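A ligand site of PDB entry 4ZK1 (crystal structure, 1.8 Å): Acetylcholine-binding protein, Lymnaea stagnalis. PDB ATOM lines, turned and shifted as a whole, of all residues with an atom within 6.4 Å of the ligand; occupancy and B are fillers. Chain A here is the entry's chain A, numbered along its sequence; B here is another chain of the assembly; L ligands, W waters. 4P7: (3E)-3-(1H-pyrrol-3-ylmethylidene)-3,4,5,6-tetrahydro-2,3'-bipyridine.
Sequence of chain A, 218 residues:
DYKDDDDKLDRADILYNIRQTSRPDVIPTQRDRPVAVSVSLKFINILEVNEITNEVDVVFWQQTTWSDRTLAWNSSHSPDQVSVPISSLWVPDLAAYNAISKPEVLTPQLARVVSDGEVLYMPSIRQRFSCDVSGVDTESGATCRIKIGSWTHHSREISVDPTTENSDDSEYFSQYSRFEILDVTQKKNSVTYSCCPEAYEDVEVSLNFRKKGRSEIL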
ATOM      1  N   TYR A  97      15.068 -17.295 -35.867  1.00  0.00           N
ATOM      2  CA  TYR A  97      14.887 -17.177 -34.421  1.00  0.00           C
ATOM      3  C   TYR A  97      14.096 -15.943 -34.013  1.00  0.00           C
ATOM      4  O   TYR A  97      13.444 -15.936 -32.961  1.00  0.00           O
ATOM      5  CB  TYR A  97      16.242 -17.130 -33.709  1.00  0.00           C
ATOM      6  CG  TYR A  97      16.963 -18.444 -33.558  1.00  0.00           C
ATOM      7  CD1 TYR A  97      17.080 -19.328 -34.617  1.00  0.00           C
ATOM      8  CD2 TYR A  97      17.554 -18.781 -32.348  1.00  0.00           C
ATOM      9  CE1 TYR A  97      17.763 -20.534 -34.472  1.00  0.00           C
ATOM     10  CE2 TYR A  97      18.230 -19.975 -32.193  1.00  0.00           C
ATOM     11  CZ  TYR A  97      18.336 -20.841 -33.252  1.00  0.00           C
ATOM     12  OH  TYR A  97      19.020 -22.025 -33.103  1.00  0.00           O
ATOM     13  N   SER A 150      18.634 -24.639 -38.049  1.00  0.00           N
ATOM     14  CA  SER A 150      17.727 -25.768 -37.856  1.00  0.00           C
ATOM     15  C   SER A 150      16.938 -25.642 -36.552  1.00  0.00           C
ATOM     16  O   SER A 150      17.503 -25.328 -35.504  1.00  0.00           O
ATOM     17  CB  SER A 150      18.493 -27.095 -37.854  1.00  0.00           C
ATOM     18  OG  SER A 150      17.617 -28.155 -37.516  1.00  0.00           O
ATOM     19  N   TRP A 151      15.638 -25.887 -36.590  1.00  0.00           N
ATOM     20  CA  TRP A 151      14.860 -25.742 -35.377  1.00  0.00           C
ATOM     21  C   TRP A 151      15.098 -26.878 -34.380  1.00  0.00           C
ATOM     22  O   TRP A 151      15.109 -26.663 -33.166  1.00  0.00           O
ATOM     23  CB  TRP A 151      13.360 -25.648 -35.704  1.00  0.00           C
ATOM     24  CG  TRP A 151      12.557 -25.258 -34.520  1.00  0.00           C
ATOM     25  CD1 TRP A 151      11.594 -25.999 -33.895  1.00  0.00           C
ATOM     26  CD2 TRP A 151      12.664 -24.025 -33.788  1.00  0.00           C
ATOM     27  NE1 TRP A 151      11.092 -25.296 -32.816  1.00  0.00           N
ATOM     28  CE2 TRP A 151      11.734 -24.082 -32.738  1.00  0.00           C
ATOM     29  CE3 TRP A 151      13.464 -22.884 -33.923  1.00  0.00           C
ATOM     30  CZ2 TRP A 151      11.566 -23.037 -31.823  1.00  0.00           C
ATOM     31  CZ3 TRP A 151      13.283 -21.842 -33.014  1.00  0.00           C
ATOM     32  CH2 TRP A 151      12.347 -21.936 -31.984  1.00  0.00           C
ATOM     33  N   THR A 152      15.320 -28.098 -34.880  1.00  0.00           N
ATOM     34  CA  THR A 152      15.370 -29.232 -33.957  1.00  0.00           C
ATOM     35  C   THR A 152      16.657 -30.036 -34.043  1.00  0.00           C
ATOM     36  O   THR A 152      16.853 -30.947 -33.240  1.00  0.00           O
ATOM     37  CB  THR A 152      14.184 -30.209 -34.175  1.00  0.00           C
ATOM     38  OG1 THR A 152      14.318 -30.889 -35.429  1.00  0.00           O
ATOM     39  CG2 THR A 152      12.845 -29.460 -34.120  1.00  0.00           C
ATOM     40  N   HIS A 153      17.524 -29.718 -34.993  1.00  0.00           N
ATOM     41  CA  HIS A 153      18.778 -30.460 -35.125  1.00  0.00           C
ATOM     42  C   HIS A 153      19.973 -29.643 -34.650  1.00  0.00           C
ATOM     43  O   HIS A 153      20.264 -28.577 -35.186  1.00  0.00           O
ATOM     44  CB  HIS A 153      18.980 -30.895 -36.568  1.00  0.00           C
ATOM     45  CG  HIS A 153      17.891 -31.777 -37.089  1.00  0.00           C
ATOM     46  ND1 HIS A 153      17.827 -33.127 -36.821  1.00  0.00           N
ATOM     47  CD2 HIS A 153      16.834 -31.506 -37.885  1.00  0.00           C
ATOM     48  CE1 HIS A 153      16.780 -33.647 -37.422  1.00  0.00           C
ATOM     49  NE2 HIS A 153      16.157 -32.690 -38.081  1.00  0.00           N
ATOM     50  N   VAL A 191      24.915 -21.048 -31.427  1.00  0.00           N
ATOM     51  CA  VAL A 191      24.063 -20.651 -30.315  1.00  0.00           C
ATOM     52  C   VAL A 191      23.953 -21.762 -29.289  1.00  0.00           C
ATOM     53  O   VAL A 191      23.780 -22.936 -29.631  1.00  0.00           O
ATOM     54  CB  VAL A 191      22.656 -20.256 -30.790  1.00  0.00           C
ATOM     55  CG1 VAL A 191      21.782 -19.899 -29.608  1.00  0.00           C
ATOM     56  CG2 VAL A 191      22.728 -19.080 -31.743  1.00  0.00           C
ATOM     57  N   TYR A 193      22.358 -22.447 -25.081  1.00  0.00           N
ATOM     58  CA  TYR A 193      21.572 -21.922 -23.985  1.00  0.00           C
ATOM     59  C   TYR A 193      22.097 -22.510 -22.695  1.00  0.00           C
ATOM     60  O   TYR A 193      22.571 -23.642 -22.685  1.00  0.00           O
ATOM     61  CB  TYR A 193      20.080 -22.224 -24.187  1.00  0.00           C
ATOM     62  CG  TYR A 193      19.518 -21.485 -25.376  1.00  0.00           C
ATOM     63  CD1 TYR A 193      19.631 -22.007 -26.663  1.00  0.00           C
ATOM     64  CD2 TYR A 193      18.909 -20.248 -25.223  1.00  0.00           C
ATOM     65  CE1 TYR A 193      19.141 -21.323 -27.757  1.00  0.00           C
ATOM     66  CE2 TYR A 193      18.416 -19.550 -26.316  1.00  0.00           C
ATOM     67  CZ  TYR A 193      18.529 -20.097 -27.574  1.00  0.00           C
ATOM     68  OH  TYR A 193      18.044 -19.405 -28.665  1.00  0.00           O
ATOM     69  N   CYS A 195      20.909 -23.742 -20.143  1.00  0.00           N
ATOM     70  CA  CYS A 195      20.232 -24.928 -19.618  1.00  0.00           C
ATOM     71  C   CYS A 195      20.796 -26.240 -20.152  1.00  0.00           C
ATOM     72  O   CYS A 195      20.755 -27.260 -19.474  1.00  0.00           O
ATOM     73  CB  CYS A 195      18.750 -24.864 -19.955  1.00  0.00           C
ATOM     74  SG  CYS A 195      18.388 -24.991 -21.740  1.00  0.00           S
ATOM     75  N   CYS A 196      21.309 -26.210 -21.373  1.00  0.00           N
ATOM     76  CA  CYS A 196      21.499 -27.437 -22.138  1.00  0.00           C
ATOM     77  C   CYS A 196      22.813 -27.465 -22.910  1.00  0.00           C
ATOM     78  O   CYS A 196      23.344 -26.412 -23.266  1.00  0.00           O
ATOM     79  CB  CYS A 196      20.310 -27.628 -23.084  1.00  0.00           C
ATOM     80  SG  CYS A 196      18.761 -26.864 -22.454  1.00  0.00           S
ATOM     81  N   TYR A 200      23.552 -24.940 -31.495  1.00  0.00           N
ATOM     82  CA  TYR A 200      22.895 -24.841 -32.775  1.00  0.00           C
ATOM     83  C   TYR A 200      23.714 -23.973 -33.696  1.00  0.00           C
ATOM     84  O   TYR A 200      24.148 -22.875 -33.318  1.00  0.00           O
ATOM     85  CB  TYR A 200      21.459 -24.302 -32.612  1.00  0.00           C
ATOM     86  CG  TYR A 200      20.602 -25.275 -31.857  1.00  0.00           C
ATOM     87  CD1 TYR A 200      20.621 -25.307 -30.468  1.00  0.00           C
ATOM     88  CD2 TYR A 200      19.821 -26.219 -32.530  1.00  0.00           C
ATOM     89  CE1 TYR A 200      19.874 -26.226 -29.758  1.00  0.00           C
ATOM     90  CE2 TYR A 200      19.061 -27.141 -31.825  1.00  0.00           C
ATOM     91  CZ  TYR A 200      19.095 -27.132 -30.434  1.00  0.00           C
ATOM     92  OH  TYR A 200      18.351 -28.050 -29.732  1.00  0.00           O
ATOM     93  N   LYS B  42       8.715 -19.583 -22.853  1.00  0.00           N
ATOM     94  CA  LYS B  42       9.837 -18.656 -22.932  1.00  0.00           C
ATOM     95  C   LYS B  42       9.391 -17.531 -23.828  1.00  0.00           C
ATOM     96  O   LYS B  42       9.263 -17.718 -25.039  1.00  0.00           O
ATOM     97  CB  LYS B  42      11.094 -19.317 -23.506  1.00  0.00           C
ATOM     98  CG  LYS B  42      11.405 -20.714 -23.009  1.00  0.00           C
ATOM     99  CD  LYS B  42      11.752 -20.741 -21.543  1.00  0.00           C
ATOM    100  CE  LYS B  42      12.190 -22.135 -21.138  1.00  0.00           C
ATOM    101  NZ  LYS B  42      12.162 -22.331 -19.667  1.00  0.00           N
ATOM    102  N   TRP B  61       8.150 -19.378 -27.015  1.00  0.00           N
ATOM    103  CA  TRP B  61       8.526 -20.762 -27.266  1.00  0.00           C
ATOM    104  C   TRP B  61       7.854 -21.626 -26.198  1.00  0.00           C
ATOM    105  O   TRP B  61       8.100 -21.436 -25.006  1.00  0.00           O
ATOM    106  CB  TRP B  61      10.047 -20.935 -27.250  1.00  0.00           C
ATOM    107  CG  TRP B  61      10.775 -20.179 -28.338  1.00  0.00           C
ATOM    108  CD1 TRP B  61      10.227 -19.486 -29.377  1.00  0.00           C
ATOM    109  CD2 TRP B  61      12.197 -20.028 -28.476  1.00  0.00           C
ATOM    110  NE1 TRP B  61      11.214 -18.923 -30.168  1.00  0.00           N
ATOM    111  CE2 TRP B  61      12.432 -19.241 -29.622  1.00  0.00           C
ATOM    112  CE3 TRP B  61      13.305 -20.485 -27.738  1.00  0.00           C
ATOM    113  CZ2 TRP B  61      13.721 -18.908 -30.052  1.00  0.00           C
ATOM    114  CZ3 TRP B  61      14.574 -20.166 -28.167  1.00  0.00           C
ATOM    115  CH2 TRP B  61      14.773 -19.374 -29.306  1.00  0.00           C
ATOM    116  N   GLN B  63       7.855 -24.665 -24.384  1.00  0.00           N
ATOM    117  CA  GLN B  63       8.655 -25.854 -24.081  1.00  0.00           C
ATOM    118  C   GLN B  63       7.785 -26.919 -23.413  1.00  0.00           C
ATOM    119  O   GLN B  63       7.425 -26.795 -22.244  1.00  0.00           O
ATOM    120  CB  GLN B  63       9.839 -25.476 -23.200  1.00  0.00           C
ATOM    121  CG  GLN B  63      10.783 -26.620 -22.908  1.00  0.00           C
ATOM    122  CD  GLN B  63      11.925 -26.158 -22.028  1.00  0.00           C
ATOM    123  OE1 GLN B  63      12.398 -25.022 -22.152  1.00  0.00           O
ATOM    124  NE2 GLN B  63      12.369 -27.028 -21.129  1.00  0.00           N
ATOM    125  N   LEU B 110       8.052 -30.431 -35.619  1.00  0.00           N
ATOM    126  CA  LEU B 110       8.869 -31.609 -35.307  1.00  0.00           C
ATOM    127  C   LEU B 110       9.100 -31.610 -33.806  1.00  0.00           C
ATOM    128  O   LEU B 110       9.324 -30.548 -33.201  1.00  0.00           O
ATOM    129  CB  LEU B 110      10.208 -31.568 -36.044  1.00  0.00           C
ATOM    130  CG  LEU B 110      10.148 -31.449 -37.564  1.00  0.00           C
ATOM    131  CD1 LEU B 110      11.547 -31.346 -38.146  1.00  0.00           C
ATOM    132  CD2 LEU B 110       9.393 -32.613 -38.147  1.00  0.00           C
ATOM    133  N   ALA B 111       9.044 -32.796 -33.208  1.00  0.00           N
ATOM    134  CA  ALA B 111       9.430 -32.982 -31.822  1.00  0.00           C
ATOM    135  C   ALA B 111      10.730 -33.764 -31.768  1.00  0.00           C
ATOM    136  O   ALA B 111      11.156 -34.347 -32.767  1.00  0.00           O
ATOM    137  CB  ALA B 111       8.340 -33.730 -31.063  1.00  0.00           C
ATOM    138  N   ARG B 112      11.381 -33.738 -30.608  1.00  0.00           N
ATOM    139  CA  ARG B 112      12.516 -34.616 -30.364  1.00  0.00           C
ATOM    140  C   ARG B 112      12.063 -35.772 -29.504  1.00  0.00           C
ATOM    141  O   ARG B 112      11.372 -35.587 -28.510  1.00  0.00           O
ATOM    142  CB  ARG B 112      13.654 -33.852 -29.681  1.00  0.00           C
ATOM    143  CG  ARG B 112      14.306 -32.818 -30.572  1.00  0.00           C
ATOM    144  CD  ARG B 112      15.100 -33.499 -31.716  1.00  0.00           C
ATOM    145  NE  ARG B 112      16.434 -33.930 -31.288  1.00  0.00           N
ATOM    146  CZ  ARG B 112      17.432 -34.218 -32.124  1.00  0.00           C
ATOM    147  NH1 ARG B 112      17.230 -34.152 -33.438  1.00  0.00           N
ATOM    148  NH2 ARG B 112      18.623 -34.572 -31.662  1.00  0.00           N
ATOM    149  N   LEU B 120      10.175 -34.026 -26.445  1.00  0.00           N
ATOM    150  CA  LEU B 120      10.264 -32.576 -26.335  1.00  0.00           C
ATOM    151  C   LEU B 120       9.686 -31.939 -27.582  1.00  0.00           C
ATOM    152  O   LEU B 120      10.158 -32.185 -28.696  1.00  0.00           O
ATOM    153  CB  LEU B 120      11.719 -32.114 -26.150  1.00  0.00           C
ATOM    154  CG  LEU B 120      11.910 -30.585 -26.313  1.00  0.00           C
ATOM    155  CD1 LEU B 120      11.117 -29.784 -25.288  1.00  0.00           C
ATOM    156  CD2 LEU B 120      13.399 -30.180 -26.300  1.00  0.00           C
ATOM    157  N   TYR B 121       8.646 -31.131 -27.397  1.00  0.00           N
ATOM    158  CA  TYR B 121       8.052 -30.379 -28.487  1.00  0.00           C
ATOM    159  C   TYR B 121       8.100 -28.913 -28.096  1.00  0.00           C
ATOM    160  O   TYR B 121       7.588 -28.541 -27.028  1.00  0.00           O
ATOM    161  CB  TYR B 121       6.608 -30.839 -28.754  1.00  0.00           C
ATOM    162  CG  TYR B 121       5.959 -30.083 -29.898  1.00  0.00           C
ATOM    163  CD1 TYR B 121       6.687 -29.791 -31.039  1.00  0.00           C
ATOM    164  CD2 TYR B 121       4.626 -29.676 -29.850  1.00  0.00           C
ATOM    165  CE1 TYR B 121       6.121 -29.115 -32.100  1.00  0.00           C
ATOM    166  CE2 TYR B 121       4.047 -28.987 -30.924  1.00  0.00           C
ATOM    167  CZ  TYR B 121       4.813 -28.725 -32.045  1.00  0.00           C
ATOM    168  OH  TYR B 121       4.298 -28.040 -33.138  1.00  0.00           O
ATOM    169  N   MET B 122       8.728 -28.066 -28.911  1.00  0.00           N
ATOM    170  CA  MET B 122       8.834 -26.649 -28.539  1.00  0.00           C
ATOM    171  C   MET B 122       8.556 -25.742 -29.725  1.00  0.00           C
ATOM    172  O   MET B 122       9.477 -25.161 -30.320  1.00  0.00           O
ATOM    173  CB  MET B 122      10.212 -26.327 -27.963  1.00  0.00           C
ATOM    174  CG  MET B 122      10.286 -24.932 -27.345  1.00  0.00           C
ATOM    175  SD  MET B 122      11.959 -24.452 -26.874  1.00  0.00           S
ATOM    176  CE  MET B 122      12.649 -23.957 -28.462  1.00  0.00           C
ATOM    177  N   PRO B 123       7.274 -25.598 -30.055  1.00  0.00           N
ATOM    178  CA  PRO B 123       6.916 -24.676 -31.139  1.00  0.00           C
ATOM    179  C   PRO B 123       7.084 -23.233 -30.705  1.00  0.00           C
ATOM    180  O   PRO B 123       6.883 -22.938 -29.517  1.00  0.00           O
ATOM    181  CB  PRO B 123       5.439 -24.986 -31.370  1.00  0.00           C
ATOM    182  CG  PRO B 123       4.941 -25.425 -30.033  1.00  0.00           C
ATOM    183  CD  PRO B 123       6.095 -26.225 -29.440  1.00  0.00           C
ATOM    184  N   TYR B 172      16.073 -15.275 -23.708  1.00  0.00           N
ATOM    185  CA  TYR B 172      15.101 -15.487 -24.779  1.00  0.00           C
ATOM    186  C   TYR B 172      14.454 -14.223 -25.324  1.00  0.00           C
ATOM    187  O   TYR B 172      14.253 -14.093 -26.527  1.00  0.00           O
ATOM    188  CB  TYR B 172      14.012 -16.438 -24.297  1.00  0.00           C
ATOM    189  CG  TYR B 172      14.549 -17.759 -23.850  1.00  0.00           C
ATOM    190  CD1 TYR B 172      14.783 -18.779 -24.766  1.00  0.00           C
ATOM    191  CD2 TYR B 172      14.840 -17.994 -22.511  1.00  0.00           C
ATOM    192  CE1 TYR B 172      15.289 -19.995 -24.355  1.00  0.00           C
ATOM    193  CE2 TYR B 172      15.342 -19.212 -22.090  1.00  0.00           C
ATOM    194  CZ  TYR B 172      15.568 -20.211 -23.017  1.00  0.00           C
ATOM    195  OH  TYR B 172      16.062 -21.423 -22.599  1.00  0.00           O
HETATM  196  C17 4P7 L   1      14.414 -29.057 -29.663  1.00  0.00           C
HETATM  197  C16 4P7 L   1      15.143 -27.891 -29.613  1.00  0.00           C
HETATM  198  C4  4P7 L   1      16.483 -23.906 -26.020  1.00  0.00           C
HETATM  199  C18 4P7 L   1      13.131 -29.023 -30.167  1.00  0.00           C
HETATM  200  C14 4P7 L   1      13.259 -26.808 -30.587  1.00  0.00           C
HETATM  201  C3  4P7 L   1      16.534 -23.935 -24.651  1.00  0.00           C
HETATM  202  C1  4P7 L   1      15.304 -25.679 -25.280  1.00  0.00           C
HETATM  203  C15 4P7 L   1      14.546 -26.745 -30.085  1.00  0.00           C
HETATM  204  C5  4P7 L   1      15.694 -25.028 -26.423  1.00  0.00           C
HETATM  205  C12 4P7 L   1      15.227 -25.455 -30.097  1.00  0.00           C
HETATM  206  C11 4P7 L   1      15.811 -24.925 -28.859  1.00  0.00           C
HETATM  207  C6  4P7 L   1      15.316 -25.426 -27.730  1.00  0.00           C
HETATM  208  C10 4P7 L   1      16.843 -23.850 -28.969  1.00  0.00           C
HETATM  209  C9  4P7 L   1      17.187 -23.654 -30.423  1.00  0.00           C
HETATM  210  C8  4P7 L   1      15.901 -23.526 -31.184  1.00  0.00           C
HETATM  211  N13 4P7 L   1      12.524 -27.924 -30.629  1.00  0.00           N
HETATM  212  N7  4P7 L   1      15.232 -24.823 -31.233  1.00  0.00           N
HETATM  213  N2  4P7 L   1      15.831 -25.010 -24.214  1.00  0.00           N
HETATM  214  O   HOH W   1       9.812 -28.245 -31.648  1.00  0.00           O
HETATM  215  O   HOH W   2      19.311 -25.658 -26.304  1.00  0.00           O
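Water W1 lies within hydrogen-bond range of O of Leu 110 of chain B (2.8 Å), N13 of the ligand (2.9 Å), N of Met 122 of chain B (2.9 Å) and NE1 of Trp 151 (3.4 Å).
The backbone carbonyl oxygen (O) of Trp 151 sits close to a nitrogen (N7) of the ligand. A nitrogen (N2) of the ligand lies within hydrogen-bond range of the side-chain sulfur (SG) of Cys 195 (3.6 Å).
The backbone carbonyl oxygen of Met 122 of chain B lies within hydrogen-bond range of the indole nitrogen of Trp 151 (3.0 Å). The backbone carbonyl oxygen of Tyr 200 sits at hydrogen-bond distance from the backbone NH of Val 191 (2.7 Å). The side-chain sulfur (SG) of Cys 195 forms a disulfide with the side-chain sulfur (SG) of Cys 196 (2.0 Å). The backbone NH (N) of Arg 112 of chain B sits at hydrogen-bond distance from the backbone carbonyl oxygen (O) of Leu 120 of chain B (2.8 Å). O of Thr 152 is in hydrogen-bond range of NH1 of Arg 112 of chain B (3.2 Å). The backbone NH of Thr 152 lies close to the side-chain hydroxyl of Ser 150, 3.5 Å away.
Tyr 97 touches the ligand. CG2 of Thr 152 touches N13 of the ligand, at 3.8 Å. Tyr 193 touches the ligand (CE1 to C10, 3.6 Å). Cys 196 touches the ligand (SG to N2, 3.9 Å). Tyr 200 touches the ligand (OH to C16, 3.2 Å). Arg 112 of chain B touches the ligand. CD2 of Leu 120 of chain B touches C17 of the ligand, 3.7 Å away. CE of Met 122 of chain B touches C6 of the ligand, 3.1 Å away. Tyr 172 of chain B touches the ligand (OH to C3, 3.3 Å). 11 residues have an atom within 4 Å of the ligand: Tyr 97, Trp 151, Thr 152, Tyr 193, Cys 195, Cys 196, Tyr 200, Arg 112 of chain B, Leu 120 of chain B, Met 122 of chain B and Tyr 172 of chain B. The nearest printed residue that does not touch the ligand is Gln 63 of chain B (4.005 Å).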
